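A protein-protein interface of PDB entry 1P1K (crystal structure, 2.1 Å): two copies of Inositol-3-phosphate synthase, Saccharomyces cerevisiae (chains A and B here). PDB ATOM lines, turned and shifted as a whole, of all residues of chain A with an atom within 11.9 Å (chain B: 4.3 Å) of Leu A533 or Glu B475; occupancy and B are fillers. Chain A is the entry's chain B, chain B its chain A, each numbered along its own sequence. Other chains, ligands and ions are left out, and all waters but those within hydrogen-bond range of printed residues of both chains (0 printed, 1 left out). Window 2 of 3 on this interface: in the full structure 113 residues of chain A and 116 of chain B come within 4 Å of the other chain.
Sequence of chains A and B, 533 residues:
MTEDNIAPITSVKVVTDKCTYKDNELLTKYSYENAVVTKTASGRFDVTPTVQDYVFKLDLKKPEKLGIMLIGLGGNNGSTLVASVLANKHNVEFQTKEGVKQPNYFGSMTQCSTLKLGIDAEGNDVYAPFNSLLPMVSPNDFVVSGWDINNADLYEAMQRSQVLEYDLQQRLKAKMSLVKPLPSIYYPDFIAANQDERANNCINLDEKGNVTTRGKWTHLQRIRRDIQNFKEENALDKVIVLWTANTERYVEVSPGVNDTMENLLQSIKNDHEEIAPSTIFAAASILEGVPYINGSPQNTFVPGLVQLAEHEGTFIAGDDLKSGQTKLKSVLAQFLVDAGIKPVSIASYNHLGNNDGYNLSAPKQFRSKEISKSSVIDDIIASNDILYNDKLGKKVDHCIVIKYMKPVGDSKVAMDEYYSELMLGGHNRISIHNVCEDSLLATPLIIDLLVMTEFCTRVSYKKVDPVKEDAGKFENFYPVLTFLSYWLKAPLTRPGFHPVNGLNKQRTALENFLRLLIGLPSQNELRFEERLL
O of Glu A530 is in hydrogen-bond range of NH1 of Arg B494, at 2.6 Å.
OH of Tyr B461 sits at hydrogen-bond distance from N of Leu A533, at 2.7 Å.
NH2 of Arg B494 lies within salt-bridge range of O of Leu A533 (3.4 Å).
N of Tyr B478 lies within hydrogen-bond range of O of Arg A531 (3.0 Å).
The guanidinium group (NH1) of Arg B494 is in hydrogen-bond range of the backbone carbonyl oxygen (O) of Leu A532, at 2.6 Å.
The side-chain hydroxyl (OH) of Tyr B461 lies within hydrogen-bond range of the backbone carbonyl oxygen (O) of Asn B476 (3.0 Å).
NZ of Lys B473 is in salt-bridge range of OE1 of Glu B475 (2.8 Å).
The backbone NH of Glu B475 is in hydrogen-bond range of the backbone carbonyl oxygen of Tyr B461 (2.6 Å).
O of Leu A526 is in hydrogen-bond range of NE of Arg A531, 2.6 Å away.
Among the printed residues, pairs that only touch across the chains: Leu A532 with Tyr B461 (3.3 Å), Leu A533 with Glu B475 (3.7 Å), Leu A533 with Asn B476 (3.7 Å), Leu A533 with Tyr B478 (3.8 Å), Glu A529 with Arg B494 (3.9 Å), Glu A530 with Tyr B478 (3.9 Å) and Leu A533 with Lys B463 (3.97 Å).
Arg A527 touches none of the printed residues of chain B.
Phe A528 touches none of the printed residues of chain B.
Printed residues of chain B within 4 Å of Glu A529: Arg B494 (3.9 Å).
Printed residues of chain B within 4 Å of Glu A530: Tyr B478 (3.9 Å) and Arg B494 (2.6 Å).
Printed residues of chain B within 4 Å of Arg A531: Tyr B478.
Of the printed residues of chain B, Leu A532 touches Tyr B461 and Arg B494.
No residue of chain A comes within 4 Å of Ser B460.
Printed residues of chain A within 4 Å of Tyr B461: Leu A532 and Leu A533.
Of the printed residues of chain A, Lys B463 touches Leu A533 (3.97 Å).
No residue of chain A comes within 4 Å of Lys B473.
No residue of chain A comes within 4 Å of Phe B474.
Glu B475 touches just one residue of chain A: Leu A533 (3.7 Å).
Tyr B478 touches just these residues of chain A: Glu A530, Arg A531 and Leu A533.
Of the 9 printed residues of chain B, 6 touch a printed residue of chain A.
Among the printed residues, 12 pairs touch across the chains.
No position is printed for both chains.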
ATOM      1  N   LEU A 526      10.426  10.490  13.469  1.00  0.00           N
ATOM      2  CA  LEU A 526      10.696  10.198  12.064  1.00  0.00           C
ATOM      3  C   LEU A 526       9.469   9.794  11.282  1.00  0.00           C
ATOM      4  O   LEU A 526       9.416   9.986  10.069  1.00  0.00           O
ATOM      5  CB  LEU A 526      11.756   9.112  11.957  1.00  0.00           C
ATOM      6  CG  LEU A 526      13.104   9.611  12.469  1.00  0.00           C
ATOM      7  CD1 LEU A 526      14.088   8.453  12.582  1.00  0.00           C
ATOM      8  CD2 LEU A 526      13.612  10.699  11.522  1.00  0.00           C
ATOM      9  N   ARG A 527       8.492   9.219  11.969  1.00  0.00           N
ATOM     10  CA  ARG A 527       7.254   8.808  11.330  1.00  0.00           C
ATOM     11  C   ARG A 527       7.475   8.207   9.945  1.00  0.00           C
ATOM     12  O   ARG A 527       6.878   8.659   8.963  1.00  0.00           O
ATOM     13  CB  ARG A 527       6.314  10.010  11.219  1.00  0.00           C
ATOM     14  CG  ARG A 527       5.928  10.606  12.559  1.00  0.00           C
ATOM     15  CD  ARG A 527       5.270  11.963  12.397  1.00  0.00           C
ATOM     16  NE  ARG A 527       4.949  12.574  13.688  1.00  0.00           N
ATOM     17  CZ  ARG A 527       3.898  12.250  14.432  1.00  0.00           C
ATOM     18  NH1 ARG A 527       3.051  11.315  14.014  1.00  0.00           N
ATOM     19  NH2 ARG A 527       3.695  12.858  15.596  1.00  0.00           N
ATOM     20  N   PHE A 528       8.327   7.190   9.864  1.00  0.00           N
ATOM     21  CA  PHE A 528       8.609   6.542   8.593  1.00  0.00           C
ATOM     22  C   PHE A 528       7.409   5.794   8.021  1.00  0.00           C
ATOM     23  O   PHE A 528       7.391   5.478   6.840  1.00  0.00           O
ATOM     24  CB  PHE A 528       9.797   5.600   8.745  1.00  0.00           C
ATOM     25  CG  PHE A 528      11.128   6.298   8.753  1.00  0.00           C
ATOM     26  CD1 PHE A 528      12.275   5.633   9.171  1.00  0.00           C
ATOM     27  CD2 PHE A 528      11.244   7.615   8.311  1.00  0.00           C
ATOM     28  CE1 PHE A 528      13.522   6.270   9.147  1.00  0.00           C
ATOM     29  CE2 PHE A 528      12.485   8.259   8.283  1.00  0.00           C
ATOM     30  CZ  PHE A 528      13.624   7.586   8.701  1.00  0.00           C
ATOM     31  N   GLU A 529       6.404   5.509   8.844  1.00  0.00           N
ATOM     32  CA  GLU A 529       5.206   4.824   8.352  1.00  0.00           C
ATOM     33  C   GLU A 529       4.478   5.732   7.357  1.00  0.00           C
ATOM     34  O   GLU A 529       3.671   5.274   6.554  1.00  0.00           O
ATOM     35  CB  GLU A 529       4.245   4.494   9.499  1.00  0.00           C
ATOM     36  CG  GLU A 529       4.739   3.456  10.490  1.00  0.00           C
ATOM     37  CD  GLU A 529       5.683   4.020  11.537  1.00  0.00           C
ATOM     38  OE1 GLU A 529       6.099   3.244  12.424  1.00  0.00           O
ATOM     39  OE2 GLU A 529       6.005   5.229  11.478  1.00  0.00           O
ATOM     40  N   GLU A 530       4.763   7.027   7.437  1.00  0.00           N
ATOM     41  CA  GLU A 530       4.149   8.005   6.556  1.00  0.00           C
ATOM     42  C   GLU A 530       5.143   8.526   5.525  1.00  0.00           C
ATOM     43  O   GLU A 530       4.879   8.487   4.327  1.00  0.00           O
ATOM     44  CB  GLU A 530       3.594   9.181   7.374  1.00  0.00           C
ATOM     45  CG  GLU A 530       3.103  10.355   6.524  1.00  0.00           C
ATOM     46  CD  GLU A 530       2.582  11.527   7.351  1.00  0.00           C
ATOM     47  OE1 GLU A 530       3.252  11.905   8.336  1.00  0.00           O
ATOM     48  OE2 GLU A 530       1.511  12.083   7.009  1.00  0.00           O
ATOM     49  N   ARG A 531       6.295   8.995   5.989  1.00  0.00           N
ATOM     50  CA  ARG A 531       7.302   9.562   5.096  1.00  0.00           C
ATOM     51  C   ARG A 531       7.855   8.628   4.030  1.00  0.00           C
ATOM     52  O   ARG A 531       8.203   9.067   2.931  1.00  0.00           O
ATOM     53  CB  ARG A 531       8.472  10.126   5.903  1.00  0.00           C
ATOM     54  CG  ARG A 531       8.092  11.201   6.898  1.00  0.00           C
ATOM     55  CD  ARG A 531       9.335  11.766   7.550  1.00  0.00           C
ATOM     56  NE  ARG A 531       9.059  12.285   8.888  1.00  0.00           N
ATOM     57  CZ  ARG A 531       8.300  13.344   9.145  1.00  0.00           C
ATOM     58  NH1 ARG A 531       7.738  14.013   8.151  1.00  0.00           N
ATOM     59  NH2 ARG A 531       8.095  13.723  10.399  1.00  0.00           N
ATOM     60  N   LEU A 532       7.953   7.345   4.353  1.00  0.00           N
ATOM     61  CA  LEU A 532       8.496   6.383   3.402  1.00  0.00           C
ATOM     62  C   LEU A 532       7.379   5.568   2.762  1.00  0.00           C
ATOM     63  O   LEU A 532       6.268   5.486   3.301  1.00  0.00           O
ATOM     64  CB  LEU A 532       9.493   5.455   4.104  1.00  0.00           C
ATOM     65  CG  LEU A 532      10.588   6.116   4.955  1.00  0.00           C
ATOM     66  CD1 LEU A 532      11.460   5.038   5.575  1.00  0.00           C
ATOM     67  CD2 LEU A 532      11.432   7.064   4.104  1.00  0.00           C
ATOM     68  N   LEU A 533       7.677   4.976   1.607  1.00  0.00           N
ATOM     69  CA  LEU A 533       6.706   4.168   0.873  1.00  0.00           C
ATOM     70  C   LEU A 533       6.383   2.892   1.633  1.00  0.00           C
ATOM     71  O   LEU A 533       5.192   2.710   1.961  1.00  0.00           O
ATOM     72  CB  LEU A 533       7.250   3.811  -0.515  1.00  0.00           C
ATOM     73  CG  LEU A 533       7.527   4.986  -1.457  1.00  0.00           C
ATOM     74  CD1 LEU A 533       8.238   4.486  -2.705  1.00  0.00           C
ATOM     75  CD2 LEU A 533       6.222   5.687  -1.807  1.00  0.00           C
ATOM     76  OXT LEU A 533       7.321   2.101   1.887  1.00  0.00           O
ATOM     77  N   SER B 460      17.536   8.141  -0.963  1.00  0.00           N
ATOM     78  CA  SER B 460      16.735   6.987  -1.352  1.00  0.00           C
ATOM     79  C   SER B 460      16.954   5.947  -0.267  1.00  0.00           C
ATOM     80  O   SER B 460      17.852   6.091   0.570  1.00  0.00           O
ATOM     81  CB  SER B 460      17.116   6.450  -2.750  1.00  0.00           C
ATOM     82  OG  SER B 460      18.443   5.962  -2.817  1.00  0.00           O
ATOM     83  N   TYR B 461      16.134   4.905  -0.271  1.00  0.00           N
ATOM     84  CA  TYR B 461      16.233   3.878   0.753  1.00  0.00           C
ATOM     85  C   TYR B 461      15.574   2.572   0.333  1.00  0.00           C
ATOM     86  O   TYR B 461      15.012   2.453  -0.754  1.00  0.00           O
ATOM     87  CB  TYR B 461      15.538   4.387   2.005  1.00  0.00           C
ATOM     88  CG  TYR B 461      14.090   4.688   1.723  1.00  0.00           C
ATOM     89  CD1 TYR B 461      13.101   3.735   1.947  1.00  0.00           C
ATOM     90  CD2 TYR B 461      13.721   5.900   1.143  1.00  0.00           C
ATOM     91  CE1 TYR B 461      11.774   3.981   1.591  1.00  0.00           C
ATOM     92  CE2 TYR B 461      12.405   6.156   0.786  1.00  0.00           C
ATOM     93  CZ  TYR B 461      11.438   5.196   1.010  1.00  0.00           C
ATOM     94  OH  TYR B 461      10.141   5.457   0.645  1.00  0.00           O
ATOM     95  N   LYS B 463      13.780  -1.162   2.447  1.00  0.00           N
ATOM     96  CA  LYS B 463      13.550  -1.940   3.654  1.00  0.00           C
ATOM     97  C   LYS B 463      14.587  -3.054   3.684  1.00  0.00           C
ATOM     98  O   LYS B 463      15.020  -3.543   2.644  1.00  0.00           O
ATOM     99  CB  LYS B 463      12.157  -2.566   3.648  1.00  0.00           C
ATOM    100  CG  LYS B 463      11.012  -1.606   3.397  1.00  0.00           C
ATOM    101  CD  LYS B 463       9.683  -2.344   3.531  1.00  0.00           C
ATOM    102  CE  LYS B 463       8.501  -1.501   3.075  1.00  0.00           C
ATOM    103  NZ  LYS B 463       7.207  -2.243   3.169  1.00  0.00           N
ATOM    104  N   LYS B 473      14.852  -3.031  -3.531  1.00  0.00           N
ATOM    105  CA  LYS B 473      15.701  -2.051  -4.201  1.00  0.00           C
ATOM    106  C   LYS B 473      15.345  -0.653  -3.691  1.00  0.00           C
ATOM    107  O   LYS B 473      14.261  -0.441  -3.139  1.00  0.00           O
ATOM    108  CB  LYS B 473      15.513  -2.147  -5.719  1.00  0.00           C
ATOM    109  CG  LYS B 473      14.099  -1.858  -6.214  1.00  0.00           C
ATOM    110  CD  LYS B 473      13.899  -0.368  -6.482  1.00  0.00           C
ATOM    111  CE  LYS B 473      12.548  -0.081  -7.132  1.00  0.00           C
ATOM    112  NZ  LYS B 473      12.385   1.361  -7.477  1.00  0.00           N
ATOM    113  N   PHE B 474      16.253   0.300  -3.875  1.00  0.00           N
ATOM    114  CA  PHE B 474      16.036   1.659  -3.402  1.00  0.00           C
ATOM    115  C   PHE B 474      14.872   2.421  -4.008  1.00  0.00           C
ATOM    116  O   PHE B 474      14.654   2.392  -5.220  1.00  0.00           O
ATOM    117  CB  PHE B 474      17.300   2.480  -3.581  1.00  0.00           C
ATOM    118  CG  PHE B 474      18.442   2.014  -2.737  1.00  0.00           C
ATOM    119  CD1 PHE B 474      19.394   1.154  -3.252  1.00  0.00           C
ATOM    120  CD2 PHE B 474      18.562   2.432  -1.424  1.00  0.00           C
ATOM    121  CE1 PHE B 474      20.459   0.718  -2.469  1.00  0.00           C
ATOM    122  CE2 PHE B 474      19.615   2.004  -0.638  1.00  0.00           C
ATOM    123  CZ  PHE B 474      20.567   1.146  -1.160  1.00  0.00           C
ATOM    124  N   GLU B 475      14.140   3.112  -3.134  1.00  0.00           N
ATOM    125  CA  GLU B 475      12.979   3.931  -3.492  1.00  0.00           C
ATOM    126  C   GLU B 475      13.267   5.382  -3.101  1.00  0.00           C
ATOM    127  O   GLU B 475      14.316   5.691  -2.540  1.00  0.00           O
ATOM    128  CB  GLU B 475      11.749   3.458  -2.718  1.00  0.00           C
ATOM    129  CG  GLU B 475      11.381   2.019  -2.946  1.00  0.00           C
ATOM    130  CD  GLU B 475      10.494   1.846  -4.152  1.00  0.00           C
ATOM    131  OE1 GLU B 475      10.888   2.283  -5.255  1.00  0.00           O
ATOM    132  OE2 GLU B 475       9.397   1.272  -3.991  1.00  0.00           O
ATOM    133  N   ASN B 476      12.332   6.274  -3.394  1.00  0.00           N
ATOM    134  CA  ASN B 476      12.510   7.664  -3.028  1.00  0.00           C
ATOM    135  C   ASN B 476      11.488   7.978  -1.974  1.00  0.00           C
ATOM    136  O   ASN B 476      10.558   7.201  -1.759  1.00  0.00           O
ATOM    137  CB  ASN B 476      12.273   8.567  -4.218  1.00  0.00           C
ATOM    138  CG  ASN B 476      13.205   8.272  -5.344  1.00  0.00           C
ATOM    139  OD1 ASN B 476      14.426   8.270  -5.171  1.00  0.00           O
ATOM    140  ND2 ASN B 476      12.646   8.021  -6.520  1.00  0.00           N
ATOM    141  N   TYR B 478       8.305   9.158  -0.026  1.00  0.00           N
ATOM    142  CA  TYR B 478       6.931   9.195  -0.515  1.00  0.00           C
ATOM    143  C   TYR B 478       6.749  10.664  -0.963  1.00  0.00           C
ATOM    144  O   TYR B 478       7.061  11.590  -0.200  1.00  0.00           O
ATOM    145  CB  TYR B 478       5.953   8.834   0.604  1.00  0.00           C
ATOM    146  CG  TYR B 478       4.534   9.267   0.324  1.00  0.00           C
ATOM    147  CD1 TYR B 478       3.999  10.392   0.946  1.00  0.00           C
ATOM    148  CD2 TYR B 478       3.742   8.585  -0.602  1.00  0.00           C
ATOM    149  CE1 TYR B 478       2.713  10.835   0.654  1.00  0.00           C
ATOM    150  CE2 TYR B 478       2.451   9.022  -0.906  1.00  0.00           C
ATOM    151  CZ  TYR B 478       1.941  10.150  -0.272  1.00  0.00           C
ATOM    152  OH  TYR B 478       0.665  10.600  -0.556  1.00  0.00           O
ATOM    153  N   ARG B 494      -0.414  12.504   4.149  1.00  0.00           N
ATOM    154  CA  ARG B 494      -0.629  11.329   3.316  1.00  0.00           C
ATOM    155  C   ARG B 494      -2.039  10.849   3.667  1.00  0.00           C
ATOM    156  O   ARG B 494      -2.500  11.034   4.794  1.00  0.00           O
ATOM    157  CB  ARG B 494       0.424  10.271   3.673  1.00  0.00           C
ATOM    158  CG  ARG B 494       0.411   8.987   2.857  1.00  0.00           C
ATOM    159  CD  ARG B 494       1.691   8.191   3.117  1.00  0.00           C
ATOM    160  NE  ARG B 494       1.726   6.914   2.403  1.00  0.00           N
ATOM    161  CZ  ARG B 494       2.798   6.130   2.317  1.00  0.00           C
ATOM    162  NH1 ARG B 494       3.937   6.478   2.895  1.00  0.00           N
ATOM    163  NH2 ARG B 494       2.732   4.992   1.649  1.00  0.00           N
